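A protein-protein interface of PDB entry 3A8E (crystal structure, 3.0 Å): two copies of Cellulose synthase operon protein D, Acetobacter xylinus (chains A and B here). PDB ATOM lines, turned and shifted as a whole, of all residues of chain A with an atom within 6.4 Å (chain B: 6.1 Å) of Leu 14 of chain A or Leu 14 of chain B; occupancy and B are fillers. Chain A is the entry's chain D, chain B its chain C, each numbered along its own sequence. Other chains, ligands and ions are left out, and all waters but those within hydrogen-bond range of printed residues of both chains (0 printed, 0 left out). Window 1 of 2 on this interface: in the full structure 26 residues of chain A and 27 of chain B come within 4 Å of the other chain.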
ATOM      1  N   PHE A  10     -33.476 -12.927  23.462  1.00  0.00           N
ATOM      2  CA  PHE A  10     -32.441 -12.557  24.428  1.00  0.00           C
ATOM      3  C   PHE A  10     -32.927 -12.420  25.855  1.00  0.00           C
ATOM      4  O   PHE A  10     -32.157 -12.064  26.752  1.00  0.00           O
ATOM      5  CB  PHE A  10     -31.753 -11.263  24.001  1.00  0.00           C
ATOM      6  CG  PHE A  10     -30.861 -11.426  22.824  1.00  0.00           C
ATOM      7  CD1 PHE A  10     -29.815 -12.340  22.857  1.00  0.00           C
ATOM      8  CD2 PHE A  10     -31.063 -10.674  21.679  1.00  0.00           C
ATOM      9  CE1 PHE A  10     -28.982 -12.500  21.765  1.00  0.00           C
ATOM     10  CE2 PHE A  10     -30.237 -10.823  20.582  1.00  0.00           C
ATOM     11  CZ  PHE A  10     -29.192 -11.739  20.623  1.00  0.00           C
ATOM     12  N   THR A  11     -34.199 -12.714  26.069  1.00  0.00           N
ATOM     13  CA  THR A  11     -34.830 -12.398  27.342  1.00  0.00           C
ATOM     14  C   THR A  11     -34.421 -13.313  28.500  1.00  0.00           C
ATOM     15  O   THR A  11     -34.206 -12.818  29.605  1.00  0.00           O
ATOM     16  CB  THR A  11     -36.354 -12.230  27.200  1.00  0.00           C
ATOM     17  OG1 THR A  11     -37.018 -12.641  28.406  1.00  0.00           O
ATOM     18  CG2 THR A  11     -36.838 -13.033  26.037  1.00  0.00           C
ATOM     19  N   LEU A  12     -34.285 -14.617  28.274  1.00  0.00           N
ATOM     20  CA  LEU A  12     -33.783 -15.482  29.347  1.00  0.00           C
ATOM     21  C   LEU A  12     -32.368 -15.061  29.719  1.00  0.00           C
ATOM     22  O   LEU A  12     -32.017 -15.014  30.898  1.00  0.00           O
ATOM     23  CB  LEU A  12     -33.798 -16.956  28.952  1.00  0.00           C
ATOM     24  CG  LEU A  12     -34.260 -17.999  29.985  1.00  0.00           C
ATOM     25  CD1 LEU A  12     -33.815 -19.378  29.514  1.00  0.00           C
ATOM     26  CD2 LEU A  12     -33.772 -17.747  31.414  1.00  0.00           C
ATOM     27  N   PHE A  13     -31.566 -14.750  28.705  1.00  0.00           N
ATOM     28  CA  PHE A  13     -30.247 -14.170  28.913  1.00  0.00           C
ATOM     29  C   PHE A  13     -30.314 -12.948  29.828  1.00  0.00           C
ATOM     30  O   PHE A  13     -29.585 -12.882  30.815  1.00  0.00           O
ATOM     31  CB  PHE A  13     -29.587 -13.821  27.574  1.00  0.00           C
ATOM     32  CG  PHE A  13     -28.277 -13.096  27.711  1.00  0.00           C
ATOM     33  CD1 PHE A  13     -27.131 -13.774  28.106  1.00  0.00           C
ATOM     34  CD2 PHE A  13     -28.192 -11.735  27.439  1.00  0.00           C
ATOM     35  CE1 PHE A  13     -25.924 -13.108  28.233  1.00  0.00           C
ATOM     36  CE2 PHE A  13     -26.990 -11.059  27.566  1.00  0.00           C
ATOM     37  CZ  PHE A  13     -25.854 -11.746  27.964  1.00  0.00           C
ATOM     38  N   LEU A  14     -31.192 -11.998  29.521  1.00  0.00           N
ATOM     39  CA  LEU A  14     -31.296 -10.793  30.346  1.00  0.00           C
ATOM     40  C   LEU A  14     -31.802 -11.077  31.757  1.00  0.00           C
ATOM     41  O   LEU A  14     -31.414 -10.389  32.698  1.00  0.00           O
ATOM     42  CB  LEU A  14     -32.141  -9.714  29.670  1.00  0.00           C
ATOM     43  CG  LEU A  14     -31.502  -9.074  28.435  1.00  0.00           C
ATOM     44  CD1 LEU A  14     -32.457  -8.084  27.827  1.00  0.00           C
ATOM     45  CD2 LEU A  14     -30.157  -8.408  28.744  1.00  0.00           C
ATOM     46  N   GLN A  15     -32.663 -12.084  31.901  1.00  0.00           N
ATOM     47  CA  GLN A  15     -33.125 -12.507  33.217  1.00  0.00           C
ATOM     48  C   GLN A  15     -31.942 -12.928  34.071  1.00  0.00           C
ATOM     49  O   GLN A  15     -31.820 -12.501  35.218  1.00  0.00           O
ATOM     50  CB  GLN A  15     -34.123 -13.657  33.111  1.00  0.00           C
ATOM     51  CG  GLN A  15     -35.501 -13.254  32.622  1.00  0.00           C
ATOM     52  CD  GLN A  15     -36.417 -14.446  32.454  1.00  0.00           C
ATOM     53  OE1 GLN A  15     -36.631 -14.924  31.339  1.00  0.00           O
ATOM     54  NE2 GLN A  15     -36.946 -14.950  33.564  1.00  0.00           N
ATOM     55  N   THR A  16     -31.064 -13.754  33.507  1.00  0.00           N
ATOM     56  CA  THR A  16     -29.876 -14.194  34.239  1.00  0.00           C
ATOM     57  C   THR A  16     -28.800 -13.108  34.326  1.00  0.00           C
ATOM     58  O   THR A  16     -28.099 -13.023  35.335  1.00  0.00           O
ATOM     59  CB  THR A  16     -29.290 -15.527  33.703  1.00  0.00           C
ATOM     60  OG1 THR A  16     -29.218 -15.486  32.274  1.00  0.00           O
ATOM     61  CG2 THR A  16     -30.161 -16.701  34.118  1.00  0.00           C
ATOM     62  N   LEU A  17     -28.685 -12.275  33.291  1.00  0.00           N
ATOM     63  CA  LEU A  17     -27.758 -11.145  33.329  1.00  0.00           C
ATOM     64  C   LEU A  17     -28.150 -10.140  34.408  1.00  0.00           C
ATOM     65  O   LEU A  17     -27.345  -9.832  35.287  1.00  0.00           O
ATOM     66  CB  LEU A  17     -27.639 -10.456  31.969  1.00  0.00           C
ATOM     67  CG  LEU A  17     -26.683  -9.262  31.875  1.00  0.00           C
ATOM     68  CD1 LEU A  17     -25.227  -9.675  32.061  1.00  0.00           C
ATOM     69  CD2 LEU A  17     -26.867  -8.566  30.548  1.00  0.00           C
ATOM     70  N   SER A  18     -29.383  -9.643  34.346  1.00  0.00           N
ATOM     71  CA  SER A  18     -29.891  -8.727  35.362  1.00  0.00           C
ATOM     72  C   SER A  18     -29.544  -9.239  36.755  1.00  0.00           C
ATOM     73  O   SER A  18     -28.940  -8.523  37.556  1.00  0.00           O
ATOM     74  CB  SER A  18     -31.404  -8.544  35.229  1.00  0.00           C
ATOM     75  OG  SER A  18     -32.093  -9.763  35.439  1.00  0.00           O
ATOM     76  N   TRP A  19     -29.917 -10.491  37.015  1.00  0.00           N
ATOM     77  CA  TRP A  19     -29.675 -11.167  38.285  1.00  0.00           C
ATOM     78  C   TRP A  19     -28.211 -11.186  38.675  1.00  0.00           C
ATOM     79  O   TRP A  19     -27.833 -10.705  39.748  1.00  0.00           O
ATOM     80  CB  TRP A  19     -30.162 -12.604  38.188  1.00  0.00           C
ATOM     81  CG  TRP A  19     -31.417 -12.867  38.926  1.00  0.00           C
ATOM     82  CD1 TRP A  19     -32.679 -12.452  38.589  1.00  0.00           C
ATOM     83  CD2 TRP A  19     -31.548 -13.627  40.127  1.00  0.00           C
ATOM     84  NE1 TRP A  19     -33.588 -12.905  39.517  1.00  0.00           N
ATOM     85  CE2 TRP A  19     -32.922 -13.631  40.470  1.00  0.00           C
ATOM     86  CE3 TRP A  19     -30.640 -14.305  40.949  1.00  0.00           C
ATOM     87  CZ2 TRP A  19     -33.407 -14.282  41.600  1.00  0.00           C
ATOM     88  CZ3 TRP A  19     -31.121 -14.954  42.071  1.00  0.00           C
ATOM     89  CH2 TRP A  19     -32.495 -14.938  42.387  1.00  0.00           C
ATOM     90  N   VAL A  37     -25.803   2.908  29.006  1.00  0.00           N
ATOM     91  CA  VAL A  37     -26.271   2.098  27.889  1.00  0.00           C
ATOM     92  C   VAL A  37     -27.478   2.778  27.230  1.00  0.00           C
ATOM     93  O   VAL A  37     -27.591   2.804  26.001  1.00  0.00           O
ATOM     94  CB  VAL A  37     -26.579   0.647  28.339  1.00  0.00           C
ATOM     95  CG1 VAL A  37     -27.227  -0.156  27.224  1.00  0.00           C
ATOM     96  CG2 VAL A  37     -25.302  -0.038  28.795  1.00  0.00           C
ATOM     97  N   VAL A  93     -37.823  -8.066  31.887  1.00  0.00           N
ATOM     98  CA  VAL A  93     -36.851  -9.153  31.811  1.00  0.00           C
ATOM     99  C   VAL A  93     -36.715  -9.887  33.151  1.00  0.00           C
ATOM    100  O   VAL A  93     -35.665  -9.862  33.793  1.00  0.00           O
ATOM    101  CB  VAL A  93     -35.474  -8.656  31.277  1.00  0.00           C
ATOM    102  CG1 VAL A  93     -35.639  -8.034  29.895  1.00  0.00           C
ATOM    103  CG2 VAL A  93     -34.835  -7.631  32.232  1.00  0.00           C
ATOM    104  N   GLY A  94     -37.789 -10.544  33.570  1.00  0.00           N
ATOM    105  CA  GLY A  94     -37.798 -11.213  34.861  1.00  0.00           C
ATOM    106  C   GLY A  94     -38.070 -10.245  35.995  1.00  0.00           C
ATOM    107  O   GLY A  94     -38.513  -9.115  35.770  1.00  0.00           O
ATOM    108  N   TRP A 103     -36.147  -3.558  35.732  1.00  0.00           N
ATOM    109  CA  TRP A 103     -34.682  -3.517  35.671  1.00  0.00           C
ATOM    110  C   TRP A 103     -34.175  -2.600  34.566  1.00  0.00           C
ATOM    111  O   TRP A 103     -33.166  -1.912  34.734  1.00  0.00           O
ATOM    112  CB  TRP A 103     -34.115  -4.933  35.468  1.00  0.00           C
ATOM    113  CG  TRP A 103     -32.616  -5.070  35.692  1.00  0.00           C
ATOM    114  CD1 TRP A 103     -31.973  -5.142  36.896  1.00  0.00           C
ATOM    115  CD2 TRP A 103     -31.589  -5.175  34.685  1.00  0.00           C
ATOM    116  NE1 TRP A 103     -30.618  -5.278  36.703  1.00  0.00           N
ATOM    117  CE2 TRP A 103     -30.353  -5.295  35.360  1.00  0.00           C
ATOM    118  CE3 TRP A 103     -31.595  -5.172  33.283  1.00  0.00           C
ATOM    119  CZ2 TRP A 103     -29.131  -5.415  34.679  1.00  0.00           C
ATOM    120  CZ3 TRP A 103     -30.376  -5.290  32.607  1.00  0.00           C
ATOM    121  CH2 TRP A 103     -29.164  -5.410  33.309  1.00  0.00           C
ATOM    122  N   LEU A 104     -34.879  -2.585  33.440  1.00  0.00           N
ATOM    123  CA  LEU A 104     -34.429  -1.812  32.289  1.00  0.00           C
ATOM    124  C   LEU A 104     -34.807  -0.336  32.338  1.00  0.00           C
ATOM    125  O   LEU A 104     -34.495   0.407  31.409  1.00  0.00           O
ATOM    126  CB  LEU A 104     -34.915  -2.449  30.986  1.00  0.00           C
ATOM    127  CG  LEU A 104     -34.146  -3.686  30.524  1.00  0.00           C
ATOM    128  CD1 LEU A 104     -34.898  -4.366  29.397  1.00  0.00           C
ATOM    129  CD2 LEU A 104     -32.752  -3.289  30.088  1.00  0.00           C
ATOM    130  N   PHE B  10     -33.912  -6.910  21.489  1.00  0.00           N
ATOM    131  CA  PHE B  10     -32.851  -6.674  22.462  1.00  0.00           C
ATOM    132  C   PHE B  10     -31.441  -6.572  21.902  1.00  0.00           C
ATOM    133  O   PHE B  10     -30.483  -6.466  22.669  1.00  0.00           O
ATOM    134  CB  PHE B  10     -32.893  -7.720  23.569  1.00  0.00           C
ATOM    135  CG  PHE B  10     -33.936  -7.455  24.601  1.00  0.00           C
ATOM    136  CD1 PHE B  10     -33.971  -6.236  25.270  1.00  0.00           C
ATOM    137  CD2 PHE B  10     -34.885  -8.420  24.913  1.00  0.00           C
ATOM    138  CE1 PHE B  10     -34.941  -5.985  26.227  1.00  0.00           C
ATOM    139  CE2 PHE B  10     -35.854  -8.175  25.871  1.00  0.00           C
ATOM    140  CZ  PHE B  10     -35.883  -6.957  26.528  1.00  0.00           C
ATOM    141  N   THR B  11     -31.307  -6.586  20.580  1.00  0.00           N
ATOM    142  CA  THR B  11     -29.979  -6.540  19.962  1.00  0.00           C
ATOM    143  C   THR B  11     -29.261  -5.219  20.204  1.00  0.00           C
ATOM    144  O   THR B  11     -28.197  -5.192  20.821  1.00  0.00           O
ATOM    145  CB  THR B  11     -30.000  -6.773  18.449  1.00  0.00           C
ATOM    146  OG1 THR B  11     -30.905  -7.836  18.123  1.00  0.00           O
ATOM    147  CG2 THR B  11     -28.602  -7.138  17.993  1.00  0.00           C
ATOM    148  N   LEU B  12     -29.849  -4.137  19.697  1.00  0.00           N
ATOM    149  CA  LEU B  12     -29.307  -2.796  19.873  1.00  0.00           C
ATOM    150  C   LEU B  12     -28.956  -2.546  21.326  1.00  0.00           C
ATOM    151  O   LEU B  12     -27.886  -2.015  21.628  1.00  0.00           O
ATOM    152  CB  LEU B  12     -30.303  -1.750  19.390  1.00  0.00           C
ATOM    153  CG  LEU B  12     -29.821  -0.304  19.440  1.00  0.00           C
ATOM    154  CD1 LEU B  12     -28.824  -0.032  18.326  1.00  0.00           C
ATOM    155  CD2 LEU B  12     -31.017   0.628  19.346  1.00  0.00           C
ATOM    156  N   PHE B  13     -29.851  -2.936  22.231  1.00  0.00           N
ATOM    157  CA  PHE B  13     -29.535  -2.850  23.642  1.00  0.00           C
ATOM    158  C   PHE B  13     -28.226  -3.590  23.922  1.00  0.00           C
ATOM    159  O   PHE B  13     -27.255  -2.986  24.382  1.00  0.00           O
ATOM    160  CB  PHE B  13     -30.667  -3.387  24.518  1.00  0.00           C
ATOM    161  CG  PHE B  13     -30.282  -3.514  25.961  1.00  0.00           C
ATOM    162  CD1 PHE B  13     -30.168  -2.379  26.764  1.00  0.00           C
ATOM    163  CD2 PHE B  13     -29.991  -4.762  26.510  1.00  0.00           C
ATOM    164  CE1 PHE B  13     -29.793  -2.487  28.093  1.00  0.00           C
ATOM    165  CE2 PHE B  13     -29.613  -4.879  27.839  1.00  0.00           C
ATOM    166  CZ  PHE B  13     -29.513  -3.739  28.635  1.00  0.00           C
ATOM    167  N   LEU B  14     -28.198  -4.885  23.618  1.00  0.00           N
ATOM    168  CA  LEU B  14     -27.012  -5.698  23.857  1.00  0.00           C
ATOM    169  C   LEU B  14     -25.791  -5.179  23.109  1.00  0.00           C
ATOM    170  O   LEU B  14     -24.678  -5.222  23.633  1.00  0.00           O
ATOM    171  CB  LEU B  14     -27.280  -7.159  23.513  1.00  0.00           C
ATOM    172  CG  LEU B  14     -28.084  -7.923  24.564  1.00  0.00           C
ATOM    173  CD1 LEU B  14     -28.240  -9.369  24.139  1.00  0.00           C
ATOM    174  CD2 LEU B  14     -27.418  -7.828  25.942  1.00  0.00           C
ATOM    175  N   GLN B  15     -26.012  -4.687  21.891  1.00  0.00           N
ATOM    176  CA  GLN B  15     -24.977  -3.997  21.131  1.00  0.00           C
ATOM    177  C   GLN B  15     -24.361  -2.885  21.957  1.00  0.00           C
ATOM    178  O   GLN B  15     -23.149  -2.870  22.164  1.00  0.00           O
ATOM    179  CB  GLN B  15     -25.536  -3.411  19.838  1.00  0.00           C
ATOM    180  CG  GLN B  15     -25.734  -4.412  18.728  1.00  0.00           C
ATOM    181  CD  GLN B  15     -26.253  -3.755  17.477  1.00  0.00           C
ATOM    182  OE1 GLN B  15     -25.494  -3.180  16.695  1.00  0.00           O
ATOM    183  NE2 GLN B  15     -27.561  -3.832  17.277  1.00  0.00           N
ATOM    184  N   THR B  16     -25.181  -1.963  22.451  1.00  0.00           N
ATOM    185  CA  THR B  16     -24.618  -0.867  23.230  1.00  0.00           C
ATOM    186  C   THR B  16     -24.221  -1.272  24.660  1.00  0.00           C
ATOM    187  O   THR B  16     -23.371  -0.616  25.264  1.00  0.00           O
ATOM    188  CB  THR B  16     -25.478   0.421  23.208  1.00  0.00           C
ATOM    189  OG1 THR B  16     -26.461   0.370  24.245  1.00  0.00           O
ATOM    190  CG2 THR B  16     -26.151   0.606  21.858  1.00  0.00           C
ATOM    191  N   LEU B  17     -24.814  -2.341  25.194  1.00  0.00           N
ATOM    192  CA  LEU B  17     -24.375  -2.851  26.491  1.00  0.00           C
ATOM    193  C   LEU B  17     -22.958  -3.415  26.382  1.00  0.00           C
ATOM    194  O   LEU B  17     -22.054  -2.970  27.094  1.00  0.00           O
ATOM    195  CB  LEU B  17     -25.343  -3.895  27.063  1.00  0.00           C
ATOM    196  CG  LEU B  17     -24.961  -4.516  28.419  1.00  0.00           C
ATOM    197  CD1 LEU B  17     -24.858  -3.472  29.520  1.00  0.00           C
ATOM    198  CD2 LEU B  17     -25.949  -5.591  28.818  1.00  0.00           C
ATOM    199  N   SER B  18     -22.767  -4.371  25.476  1.00  0.00           N
ATOM    200  CA  SER B  18     -21.464  -5.008  25.281  1.00  0.00           C
ATOM    201  C   SER B  18     -20.334  -3.990  25.092  1.00  0.00           C
ATOM    202  O   SER B  18     -19.222  -4.199  25.578  1.00  0.00           O
ATOM    203  CB  SER B  18     -21.505  -5.974  24.094  1.00  0.00           C
ATOM    204  OG  SER B  18     -21.514  -5.282  22.857  1.00  0.00           O
ATOM    205  N   TRP B  19     -20.639  -2.898  24.390  1.00  0.00           N
ATOM    206  CA  TRP B  19     -19.697  -1.805  24.150  1.00  0.00           C
ATOM    207  C   TRP B  19     -19.316  -1.148  25.465  1.00  0.00           C
ATOM    208  O   TRP B  19     -18.128  -0.976  25.757  1.00  0.00           O
ATOM    209  CB  TRP B  19     -20.339  -0.766  23.230  1.00  0.00           C
ATOM    210  CG  TRP B  19     -19.380   0.124  22.468  1.00  0.00           C
ATOM    211  CD1 TRP B  19     -18.840   1.312  22.889  1.00  0.00           C
ATOM    212  CD2 TRP B  19     -18.887  -0.088  21.137  1.00  0.00           C
ATOM    213  NE1 TRP B  19     -18.033   1.842  21.906  1.00  0.00           N
ATOM    214  CE2 TRP B  19     -18.046   1.006  20.820  1.00  0.00           C
ATOM    215  CE3 TRP B  19     -19.070  -1.099  20.184  1.00  0.00           C
ATOM    216  CZ2 TRP B  19     -17.385   1.114  19.590  1.00  0.00           C
ATOM    217  CZ3 TRP B  19     -18.414  -0.991  18.960  1.00  0.00           C
ATOM    218  CH2 TRP B  19     -17.578   0.109  18.677  1.00  0.00           C
ATOM    219  N   VAL B  93     -24.137  -9.923  18.546  1.00  0.00           N
ATOM    220  CA  VAL B  93     -24.578  -8.655  19.143  1.00  0.00           C
ATOM    221  C   VAL B  93     -23.585  -7.514  18.912  1.00  0.00           C
ATOM    222  O   VAL B  93     -22.890  -7.075  19.830  1.00  0.00           O
ATOM    223  CB  VAL B  93     -24.902  -8.782  20.660  1.00  0.00           C
ATOM    224  CG1 VAL B  93     -26.239  -9.492  20.869  1.00  0.00           C
ATOM    225  CG2 VAL B  93     -23.762  -9.466  21.424  1.00  0.00           C
ATOM    226  N   TRP B 103     -18.925 -11.756  21.098  1.00  0.00           N
ATOM    227  CA  TRP B 103     -19.024 -11.368  22.507  1.00  0.00           C
ATOM    228  C   TRP B 103     -19.769 -12.381  23.393  1.00  0.00           C
ATOM    229  O   TRP B 103     -19.294 -12.724  24.475  1.00  0.00           O
ATOM    230  CB  TRP B 103     -19.670  -9.979  22.589  1.00  0.00           C
ATOM    231  CG  TRP B 103     -19.596  -9.274  23.918  1.00  0.00           C
ATOM    232  CD1 TRP B 103     -18.552  -8.536  24.401  1.00  0.00           C
ATOM    233  CD2 TRP B 103     -20.634  -9.192  24.903  1.00  0.00           C
ATOM    234  NE1 TRP B 103     -18.868  -8.014  25.635  1.00  0.00           N
ATOM    235  CE2 TRP B 103     -20.139  -8.404  25.969  1.00  0.00           C
ATOM    236  CE3 TRP B 103     -21.930  -9.715  24.993  1.00  0.00           C
ATOM    237  CZ2 TRP B 103     -20.898  -8.128  27.118  1.00  0.00           C
ATOM    238  CZ3 TRP B 103     -22.685  -9.444  26.135  1.00  0.00           C
ATOM    239  CH2 TRP B 103     -22.164  -8.656  27.182  1.00  0.00           C
ATOM    240  N   LEU B 104     -20.920 -12.864  22.932  1.00  0.00           N
ATOM    241  CA  LEU B 104     -21.718 -13.809  23.714  1.00  0.00           C
ATOM    242  C   LEU B 104     -21.091 -15.195  23.877  1.00  0.00           C
ATOM    243  O   LEU B 104     -21.691 -16.074  24.498  1.00  0.00           O
ATOM    244  CB  LEU B 104     -23.116 -13.975  23.113  1.00  0.00           C
ATOM    245  CG  LEU B 104     -24.347 -13.282  23.701  1.00  0.00           C
ATOM    246  CD1 LEU B 104     -24.084 -12.661  25.066  1.00  0.00           C
ATOM    247  CD2 LEU B 104     -24.865 -12.243  22.740  1.00  0.00           C
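Leu 14 of chain A touches just these residues of chain B: Phe 10 (3.5 Å), Phe 13 (3.7 Å) and Leu 14 (3.96 Å).
Leu 14 of chain B touches just these residues of chain A: Phe 10, Phe 13 and Leu 14.
Printed residues of chain B within 4 Å of Phe 10 of chain A: Phe 10, Thr 11, Leu 14 and Val 93.
Of the printed residues of chain A, Val 93 of chain B touches Phe 10 (3.7 Å).
Printed residues of chain A within 4 Å of Phe 13 of chain B: Leu 14, Val 37 and Leu 104.
Leu 12 of chain B touches none of the printed residues of chain A.
The nearest residue of chain A that does not touch Leu 14 of chain B is Leu 17 of chain A (4.7 Å).
Of the 15 printed residues of chain A, 7 touch a printed residue of chain B.
Among the printed residues, no Asp or Glu carboxylate lies within 4 Å of a Lys or Arg side-chain nitrogen of the other chain.
O of Phe 13 of chain B is in hydrogen-bond range of OG1 of Thr 16 of chain B.
OG of Ser 18 of chain B sits at hydrogen-bond distance from O of Leu 14 of chain B (3.3 Å).
The backbone carbonyl oxygen (O) of Leu 14 of chain A is in hydrogen-bond range of the side-chain hydroxyl (OG) of Ser 18 of chain A (2.9 Å).
The backbone carbonyl oxygen of Phe 13 of chain A is in hydrogen-bond range of the side-chain hydroxyl of Thr 16 of chain A.
Phe 10 of chain A touches its own counterpart, Phe 10 of chain B.
Phe 10 of chain A touches Leu 14 of chain B, and with the chains exchanged Leu 14 of chain A touches Phe 10 of chain B.
Phe 13 of chain A touches Leu 104 of chain B, and with the chains exchanged Leu 104 of chain A touches Phe 13 of chain B.
Leu 104 of chain A touches Phe 10 of chain B, but with the chains exchanged Phe 10 of chain A does not touch Leu 104 of chain B (4.2 Å).
Of the 16 pairs that touch across the chains among the printed residues, 11 have their exchanged pair printed and touching as well.
Among the printed residues, pairs that only touch across the chains: Phe 10 of chain A with Phe 10 of chain B, Phe 10 of chain A with Thr 11 of chain B, Phe 10 of chain A with Leu 14 of chain B, Phe 10 of chain A with Val 93 of chain B, Phe 13 of chain A with Leu 14 of chain B, Phe 13 of chain A with Leu 104 of chain B, Leu 14 of chain A with Phe 10 of chain B, Leu 14 of chain A with Phe 13 of chain B, Leu 14 of chain A with Leu 14 of chain B, Leu 17 of chain A with Leu 17 of chain B, Val 37 of chain A with Phe 13 of chain B, Val 37 of chain A with Leu 17 of chain B, Val 93 of chain A with Phe 10 of chain B, Leu 104 of chain A with Phe 10 of chain B and Leu 104 of chain A with Phe 13 of chain B.
The side-chain hydroxyl of Thr 16 of chain B lies close to the backbone carbonyl oxygen of Val 37 of chain A.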
